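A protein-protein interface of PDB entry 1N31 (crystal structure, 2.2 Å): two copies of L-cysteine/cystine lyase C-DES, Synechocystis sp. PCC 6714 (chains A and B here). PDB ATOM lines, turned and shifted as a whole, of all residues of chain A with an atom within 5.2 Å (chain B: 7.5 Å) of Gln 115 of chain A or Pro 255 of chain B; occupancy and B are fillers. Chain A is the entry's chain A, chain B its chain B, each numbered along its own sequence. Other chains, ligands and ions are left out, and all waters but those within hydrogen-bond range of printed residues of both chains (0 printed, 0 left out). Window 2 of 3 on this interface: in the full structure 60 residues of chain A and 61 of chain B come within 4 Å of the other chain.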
ATOM      1  N   PRO A 108      20.992  12.818  16.286  1.00  0.00           N
ATOM      2  CA  PRO A 108      20.989  12.559  17.733  1.00  0.00           C
ATOM      3  C   PRO A 108      20.713  13.802  18.586  1.00  0.00           C
ATOM      4  O   PRO A 108      20.195  13.699  19.697  1.00  0.00           O
ATOM      5  CB  PRO A 108      22.378  11.970  17.987  1.00  0.00           C
ATOM      6  CG  PRO A 108      23.211  12.551  16.869  1.00  0.00           C
ATOM      7  CD  PRO A 108      22.282  12.451  15.685  1.00  0.00           C
ATOM      8  N   ILE A 111      16.827  14.213  18.656  1.00  0.00           N
ATOM      9  CA  ILE A 111      16.282  13.197  19.543  1.00  0.00           C
ATOM     10  C   ILE A 111      16.507  13.642  21.012  1.00  0.00           C
ATOM     11  O   ILE A 111      15.641  13.455  21.878  1.00  0.00           O
ATOM     12  CB  ILE A 111      16.997  11.819  19.313  1.00  0.00           C
ATOM     13  CG1 ILE A 111      16.727  11.298  17.887  1.00  0.00           C
ATOM     14  CG2 ILE A 111      16.525  10.817  20.371  1.00  0.00           C
ATOM     15  CD1 ILE A 111      17.503  10.003  17.530  1.00  0.00           C
ATOM     16  N   ALA A 112      17.664  14.240  21.292  1.00  0.00           N
ATOM     17  CA  ALA A 112      17.955  14.688  22.657  1.00  0.00           C
ATOM     18  C   ALA A 112      16.953  15.740  23.152  1.00  0.00           C
ATOM     19  O   ALA A 112      16.574  15.743  24.324  1.00  0.00           O
ATOM     20  CB  ALA A 112      19.390  15.235  22.749  1.00  0.00           C
ATOM     21  N   ILE A 113      16.521  16.632  22.265  1.00  0.00           N
ATOM     22  CA  ILE A 113      15.539  17.645  22.653  1.00  0.00           C
ATOM     23  C   ILE A 113      14.212  16.950  22.999  1.00  0.00           C
ATOM     24  O   ILE A 113      13.586  17.245  24.022  1.00  0.00           O
ATOM     25  CB  ILE A 113      15.241  18.638  21.520  1.00  0.00           C
ATOM     26  CG1 ILE A 113      16.522  19.309  21.034  1.00  0.00           C
ATOM     27  CG2 ILE A 113      14.249  19.701  22.021  1.00  0.00           C
ATOM     28  CD1 ILE A 113      16.308  20.215  19.848  1.00  0.00           C
ATOM     29  N   VAL A 114      13.779  16.047  22.125  1.00  0.00           N
ATOM     30  CA  VAL A 114      12.546  15.299  22.347  1.00  0.00           C
ATOM     31  C   VAL A 114      12.564  14.567  23.699  1.00  0.00           C
ATOM     32  O   VAL A 114      11.558  14.515  24.374  1.00  0.00           O
ATOM     33  CB  VAL A 114      12.319  14.270  21.220  1.00  0.00           C
ATOM     34  CG1 VAL A 114      11.078  13.406  21.530  1.00  0.00           C
ATOM     35  CG2 VAL A 114      12.154  15.013  19.863  1.00  0.00           C
ATOM     36  N   GLN A 115      13.710  14.023  24.098  1.00  0.00           N
ATOM     37  CA  GLN A 115      13.800  13.302  25.376  1.00  0.00           C
ATOM     38  C   GLN A 115      13.673  14.302  26.519  1.00  0.00           C
ATOM     39  O   GLN A 115      13.067  14.018  27.547  1.00  0.00           O
ATOM     40  CB  GLN A 115      15.135  12.543  25.484  1.00  0.00           C
ATOM     41  CG  GLN A 115      15.403  11.586  24.314  1.00  0.00           C
ATOM     42  CD  GLN A 115      16.714  10.833  24.444  1.00  0.00           C
ATOM     43  OE1 GLN A 115      17.704  11.375  24.915  1.00  0.00           O
ATOM     44  NE2 GLN A 115      16.726   9.586  24.010  1.00  0.00           N
ATOM     45  N   ALA A 116      14.260  15.475  26.336  1.00  0.00           N
ATOM     46  CA  ALA A 116      14.190  16.528  27.341  1.00  0.00           C
ATOM     47  C   ALA A 116      12.735  17.001  27.477  1.00  0.00           C
ATOM     48  O   ALA A 116      12.276  17.300  28.568  1.00  0.00           O
ATOM     49  CB  ALA A 116      15.073  17.687  26.939  1.00  0.00           C
ATOM     50  N   ILE A 117      12.017  17.069  26.363  1.00  0.00           N
ATOM     51  CA  ILE A 117      10.624  17.487  26.383  1.00  0.00           C
ATOM     52  C   ILE A 117       9.770  16.424  27.069  1.00  0.00           C
ATOM     53  O   ILE A 117       8.938  16.744  27.901  1.00  0.00           O
ATOM     54  CB  ILE A 117      10.051  17.678  24.947  1.00  0.00           C
ATOM     55  CG1 ILE A 117      10.748  18.832  24.237  1.00  0.00           C
ATOM     56  CG2 ILE A 117       8.544  17.915  25.015  1.00  0.00           C
ATOM     57  CD1 ILE A 117      10.623  20.155  24.958  1.00  0.00           C
ATOM     58  N   ALA A 118       9.968  15.165  26.692  1.00  0.00           N
ATOM     59  CA  ALA A 118       9.217  14.059  27.272  1.00  0.00           C
ATOM     60  C   ALA A 118       9.323  14.094  28.785  1.00  0.00           C
ATOM     61  O   ALA A 118       8.328  13.960  29.488  1.00  0.00           O
ATOM     62  CB  ALA A 118       9.748  12.713  26.746  1.00  0.00           C
ATOM     63  N   ALA A 119      10.542  14.278  29.279  1.00  0.00           N
ATOM     64  CA  ALA A 119      10.778  14.319  30.710  1.00  0.00           C
ATOM     65  C   ALA A 119      10.161  15.550  31.383  1.00  0.00           C
ATOM     66  O   ALA A 119       9.849  15.519  32.571  1.00  0.00           O
ATOM     67  CB  ALA A 119      12.265  14.285  30.979  1.00  0.00           C
ATOM     68  N   ARG A 120       9.972  16.633  30.631  1.00  0.00           N
ATOM     69  CA  ARG A 120       9.426  17.863  31.210  1.00  0.00           C
ATOM     70  C   ARG A 120       7.908  17.962  31.188  1.00  0.00           C
ATOM     71  O   ARG A 120       7.304  18.481  32.118  1.00  0.00           O
ATOM     72  CB  ARG A 120       9.985  19.093  30.491  1.00  0.00           C
ATOM     73  CG  ARG A 120      10.238  20.290  31.406  1.00  0.00           C
ATOM     74  CD  ARG A 120      11.532  20.092  32.219  1.00  0.00           C
ATOM     75  NE  ARG A 120      12.719  20.644  31.554  1.00  0.00           N
ATOM     76  CZ  ARG A 120      13.009  21.942  31.515  1.00  0.00           C
ATOM     77  NH1 ARG A 120      12.197  22.815  32.109  1.00  0.00           N
ATOM     78  NH2 ARG A 120      14.096  22.368  30.877  1.00  0.00           N
ATOM     79  N   TYR A 125       7.321   9.484  22.957  1.00  0.00           N
ATOM     80  CA  TYR A 125       7.798   9.493  21.584  1.00  0.00           C
ATOM     81  C   TYR A 125       8.208   8.093  21.135  1.00  0.00           C
ATOM     82  O   TYR A 125       8.606   7.256  21.953  1.00  0.00           O
ATOM     83  CB  TYR A 125       9.004  10.414  21.453  1.00  0.00           C
ATOM     84  CG  TYR A 125      10.250   9.866  22.103  1.00  0.00           C
ATOM     85  CD1 TYR A 125      11.162   9.100  21.379  1.00  0.00           C
ATOM     86  CD2 TYR A 125      10.517  10.110  23.448  1.00  0.00           C
ATOM     87  CE1 TYR A 125      12.327   8.589  21.981  1.00  0.00           C
ATOM     88  CE2 TYR A 125      11.673   9.606  24.060  1.00  0.00           C
ATOM     89  CZ  TYR A 125      12.573   8.851  23.317  1.00  0.00           C
ATOM     90  OH  TYR A 125      13.732   8.399  23.909  1.00  0.00           O
ATOM     91  N   VAL B 242      18.841  22.145  23.861  1.00  0.00           N
ATOM     92  CA  VAL B 242      19.972  21.229  23.730  1.00  0.00           C
ATOM     93  C   VAL B 242      20.228  20.820  22.297  1.00  0.00           C
ATOM     94  O   VAL B 242      19.413  21.084  21.413  1.00  0.00           O
ATOM     95  CB  VAL B 242      19.767  19.950  24.583  1.00  0.00           C
ATOM     96  CG1 VAL B 242      19.880  20.286  26.056  1.00  0.00           C
ATOM     97  CG2 VAL B 242      18.427  19.348  24.283  1.00  0.00           C
ATOM     98  N   ILE B 247      25.205  16.393  24.706  1.00  0.00           N
ATOM     99  CA  ILE B 247      25.255  15.018  25.175  1.00  0.00           C
ATOM    100  C   ILE B 247      26.504  14.164  24.921  1.00  0.00           C
ATOM    101  O   ILE B 247      27.473  14.588  24.282  1.00  0.00           O
ATOM    102  CB  ILE B 247      24.046  14.227  24.601  1.00  0.00           C
ATOM    103  CG1 ILE B 247      24.287  13.884  23.134  1.00  0.00           C
ATOM    104  CG2 ILE B 247      22.779  15.037  24.696  1.00  0.00           C
ATOM    105  CD1 ILE B 247      24.242  15.015  22.216  1.00  0.00           C
ATOM    106  N   THR B 248      26.468  12.955  25.481  1.00  0.00           N
ATOM    107  CA  THR B 248      27.512  11.965  25.270  1.00  0.00           C
ATOM    108  C   THR B 248      26.823  10.972  24.310  1.00  0.00           C
ATOM    109  O   THR B 248      25.586  10.962  24.194  1.00  0.00           O
ATOM    110  CB  THR B 248      27.937  11.257  26.587  1.00  0.00           C
ATOM    111  OG1 THR B 248      26.774  10.808  27.296  1.00  0.00           O
ATOM    112  CG2 THR B 248      28.759  12.212  27.458  1.00  0.00           C
ATOM    113  N   TYR B 249      27.621  10.162  23.617  1.00  0.00           N
ATOM    114  CA  TYR B 249      27.113   9.222  22.625  1.00  0.00           C
ATOM    115  C   TYR B 249      27.407   7.752  22.866  1.00  0.00           C
ATOM    116  O   TYR B 249      28.393   7.402  23.514  1.00  0.00           O
ATOM    117  CB  TYR B 249      27.673   9.579  21.253  1.00  0.00           C
ATOM    118  CG  TYR B 249      27.271  10.945  20.781  1.00  0.00           C
ATOM    119  CD1 TYR B 249      27.962  12.092  21.197  1.00  0.00           C
ATOM    120  CD2 TYR B 249      26.190  11.094  19.922  1.00  0.00           C
ATOM    121  CE1 TYR B 249      27.577  13.361  20.757  1.00  0.00           C
ATOM    122  CE2 TYR B 249      25.794  12.340  19.479  1.00  0.00           C
ATOM    123  CZ  TYR B 249      26.483  13.464  19.892  1.00  0.00           C
ATOM    124  OH  TYR B 249      26.066  14.677  19.421  1.00  0.00           O
ATOM    125  N   GLY B 250      26.553   6.899  22.305  1.00  0.00           N
ATOM    126  CA  GLY B 250      26.714   5.463  22.446  1.00  0.00           C
ATOM    127  C   GLY B 250      27.366   4.785  21.249  1.00  0.00           C
ATOM    128  O   GLY B 250      27.770   5.443  20.280  1.00  0.00           O
ATOM    129  N   LYS B 252      26.182   3.089  18.781  1.00  0.00           N
ATOM    130  CA  LYS B 252      25.557   3.343  17.480  1.00  0.00           C
ATOM    131  C   LYS B 252      25.342   4.818  17.192  1.00  0.00           C
ATOM    132  O   LYS B 252      24.626   5.154  16.253  1.00  0.00           O
ATOM    133  CB  LYS B 252      24.213   2.622  17.372  1.00  0.00           C
ATOM    134  CG  LYS B 252      24.335   1.124  17.125  1.00  0.00           C
ATOM    135  CD  LYS B 252      22.968   0.459  17.022  1.00  0.00           C
ATOM    136  CE  LYS B 252      22.165   0.967  15.833  1.00  0.00           C
ATOM    137  NZ  LYS B 252      20.873   0.221  15.658  1.00  0.00           N
ATOM    138  N   GLY B 253      25.955   5.688  17.998  1.00  0.00           N
ATOM    139  CA  GLY B 253      25.818   7.127  17.801  1.00  0.00           C
ATOM    140  C   GLY B 253      24.598   7.759  18.457  1.00  0.00           C
ATOM    141  O   GLY B 253      24.277   8.922  18.202  1.00  0.00           O
ATOM    142  N   GLU B 254      23.914   7.001  19.309  1.00  0.00           N
ATOM    143  CA  GLU B 254      22.724   7.507  19.991  1.00  0.00           C
ATOM    144  C   GLU B 254      23.068   8.216  21.298  1.00  0.00           C
ATOM    145  O   GLU B 254      24.125   7.972  21.882  1.00  0.00           O
ATOM    146  CB  GLU B 254      21.752   6.361  20.272  1.00  0.00           C
ATOM    147  CG  GLU B 254      22.181   5.365  21.371  1.00  0.00           C
ATOM    148  CD  GLU B 254      23.452   4.577  21.034  1.00  0.00           C
ATOM    149  OE1 GLU B 254      23.827   4.496  19.840  1.00  0.00           O
ATOM    150  OE2 GLU B 254      24.072   4.014  21.969  1.00  0.00           O
ATOM    151  N   PRO B 255      22.186   9.122  21.761  1.00  0.00           N
ATOM    152  CA  PRO B 255      22.386   9.876  23.008  1.00  0.00           C
ATOM    153  C   PRO B 255      22.380   8.929  24.205  1.00  0.00           C
ATOM    154  O   PRO B 255      21.504   8.075  24.314  1.00  0.00           O
ATOM    155  CB  PRO B 255      21.185  10.826  23.041  1.00  0.00           C
ATOM    156  CG  PRO B 255      20.843  11.007  21.604  1.00  0.00           C
ATOM    157  CD  PRO B 255      21.013   9.627  21.031  1.00  0.00           C
ATOM    158  N   THR B 256      23.345   9.077  25.103  1.00  0.00           N
ATOM    159  CA  THR B 256      23.414   8.208  26.273  1.00  0.00           C
ATOM    160  C   THR B 256      23.445   8.959  27.610  1.00  0.00           C
ATOM    161  O   THR B 256      23.468   8.336  28.665  1.00  0.00           O
ATOM    162  CB  THR B 256      24.656   7.306  26.217  1.00  0.00           C
ATOM    163  OG1 THR B 256      25.832   8.115  26.157  1.00  0.00           O
ATOM    164  CG2 THR B 256      24.609   6.394  25.003  1.00  0.00           C
ATOM    165  N   GLY B 257      23.446  10.288  27.563  1.00  0.00           N
ATOM    166  CA  GLY B 257      23.484  11.067  28.785  1.00  0.00           C
ATOM    167  C   GLY B 257      23.946  12.498  28.530  1.00  0.00           C
ATOM    168  O   GLY B 257      24.186  12.888  27.385  1.00  0.00           O
ATOM    169  N   TRP B 258      24.089  13.278  29.592  1.00  0.00           N
ATOM    170  CA  TRP B 258      24.497  14.653  29.436  1.00  0.00           C
ATOM    171  C   TRP B 258      26.006  14.804  29.361  1.00  0.00           C
ATOM    172  O   TRP B 258      26.754  14.044  29.982  1.00  0.00           O
ATOM    173  CB  TRP B 258      23.934  15.498  30.581  1.00  0.00           C
ATOM    174  CG  TRP B 258      22.419  15.570  30.577  1.00  0.00           C
ATOM    175  CD1 TRP B 258      21.584  15.211  31.586  1.00  0.00           C
ATOM    176  CD2 TRP B 258      21.587  16.075  29.528  1.00  0.00           C
ATOM    177  NE1 TRP B 258      20.283  15.464  31.245  1.00  0.00           N
ATOM    178  CE2 TRP B 258      20.250  15.997  29.984  1.00  0.00           C
ATOM    179  CE3 TRP B 258      21.835  16.585  28.251  1.00  0.00           C
ATOM    180  CZ2 TRP B 258      19.163  16.418  29.203  1.00  0.00           C
ATOM    181  CZ3 TRP B 258      20.754  16.999  27.478  1.00  0.00           C
ATOM    182  CH2 TRP B 258      19.439  16.913  27.957  1.00  0.00           C
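Pro 108 of chain A touches Tyr 249 of chain B. Pro 108 of chain A touches Gly 253 of chain B. Pro 108 of chain A touches Pro 255 of chain B (O to CG, 3.4 Å). CB of Ala 112 of chain A touches CG2 of Ile 247 of chain B, 3.9 Å away. O of Val 242 of chain B touches CG1 of Ile 113 of chain A (3.4 Å). Gln 115 of chain A touches Pro 255 of chain B (OE1 to CB, 3.99 Å).
No position is printed for both chains. Of the 6 pairs that touch across the chains among the printed residues, none has its exchanged pair printed and touching as well.
NE2 of Gln 115 of chain A lies within hydrogen-bond range of OH of Tyr 125 of chain A, 3.2 Å away.
Hydrophobic or aromatic side chains of chain A that line the printed part of chain B: Pro 108, Ala 112 and Ile 113. Of the 12 printed residues of chain B, 5 touch a printed residue of chain A. Among the printed residues, 6 pairs touch across the chains.
Printed residues of chain B within 4 Å of Pro 108 of chain A: Tyr 249 (3.7 Å), Gly 253 (3.6 Å) and Pro 255 (3.4 Å). Of the printed residues of chain B, Ala 112 of chain A touches Ile 247 (3.9 Å). Of the printed residues of chain B, Gln 115 of chain A touches Pro 255. Thr 248 of chain B touches none of the printed residues of chain A. Of the printed residues of chain A, Tyr 249 of chain B touches Pro 108. Of the printed residues of chain A, Gly 253 of chain B touches Pro 108. Printed residues of chain A within 4 Å of Pro 255 of chain B: Pro 108 (3.4 Å) and Gln 115 (3.99 Å). The nearest printed residue of chain A that does not touch Gly 253 of chain B is Ile 111 of chain A (6.9 Å).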
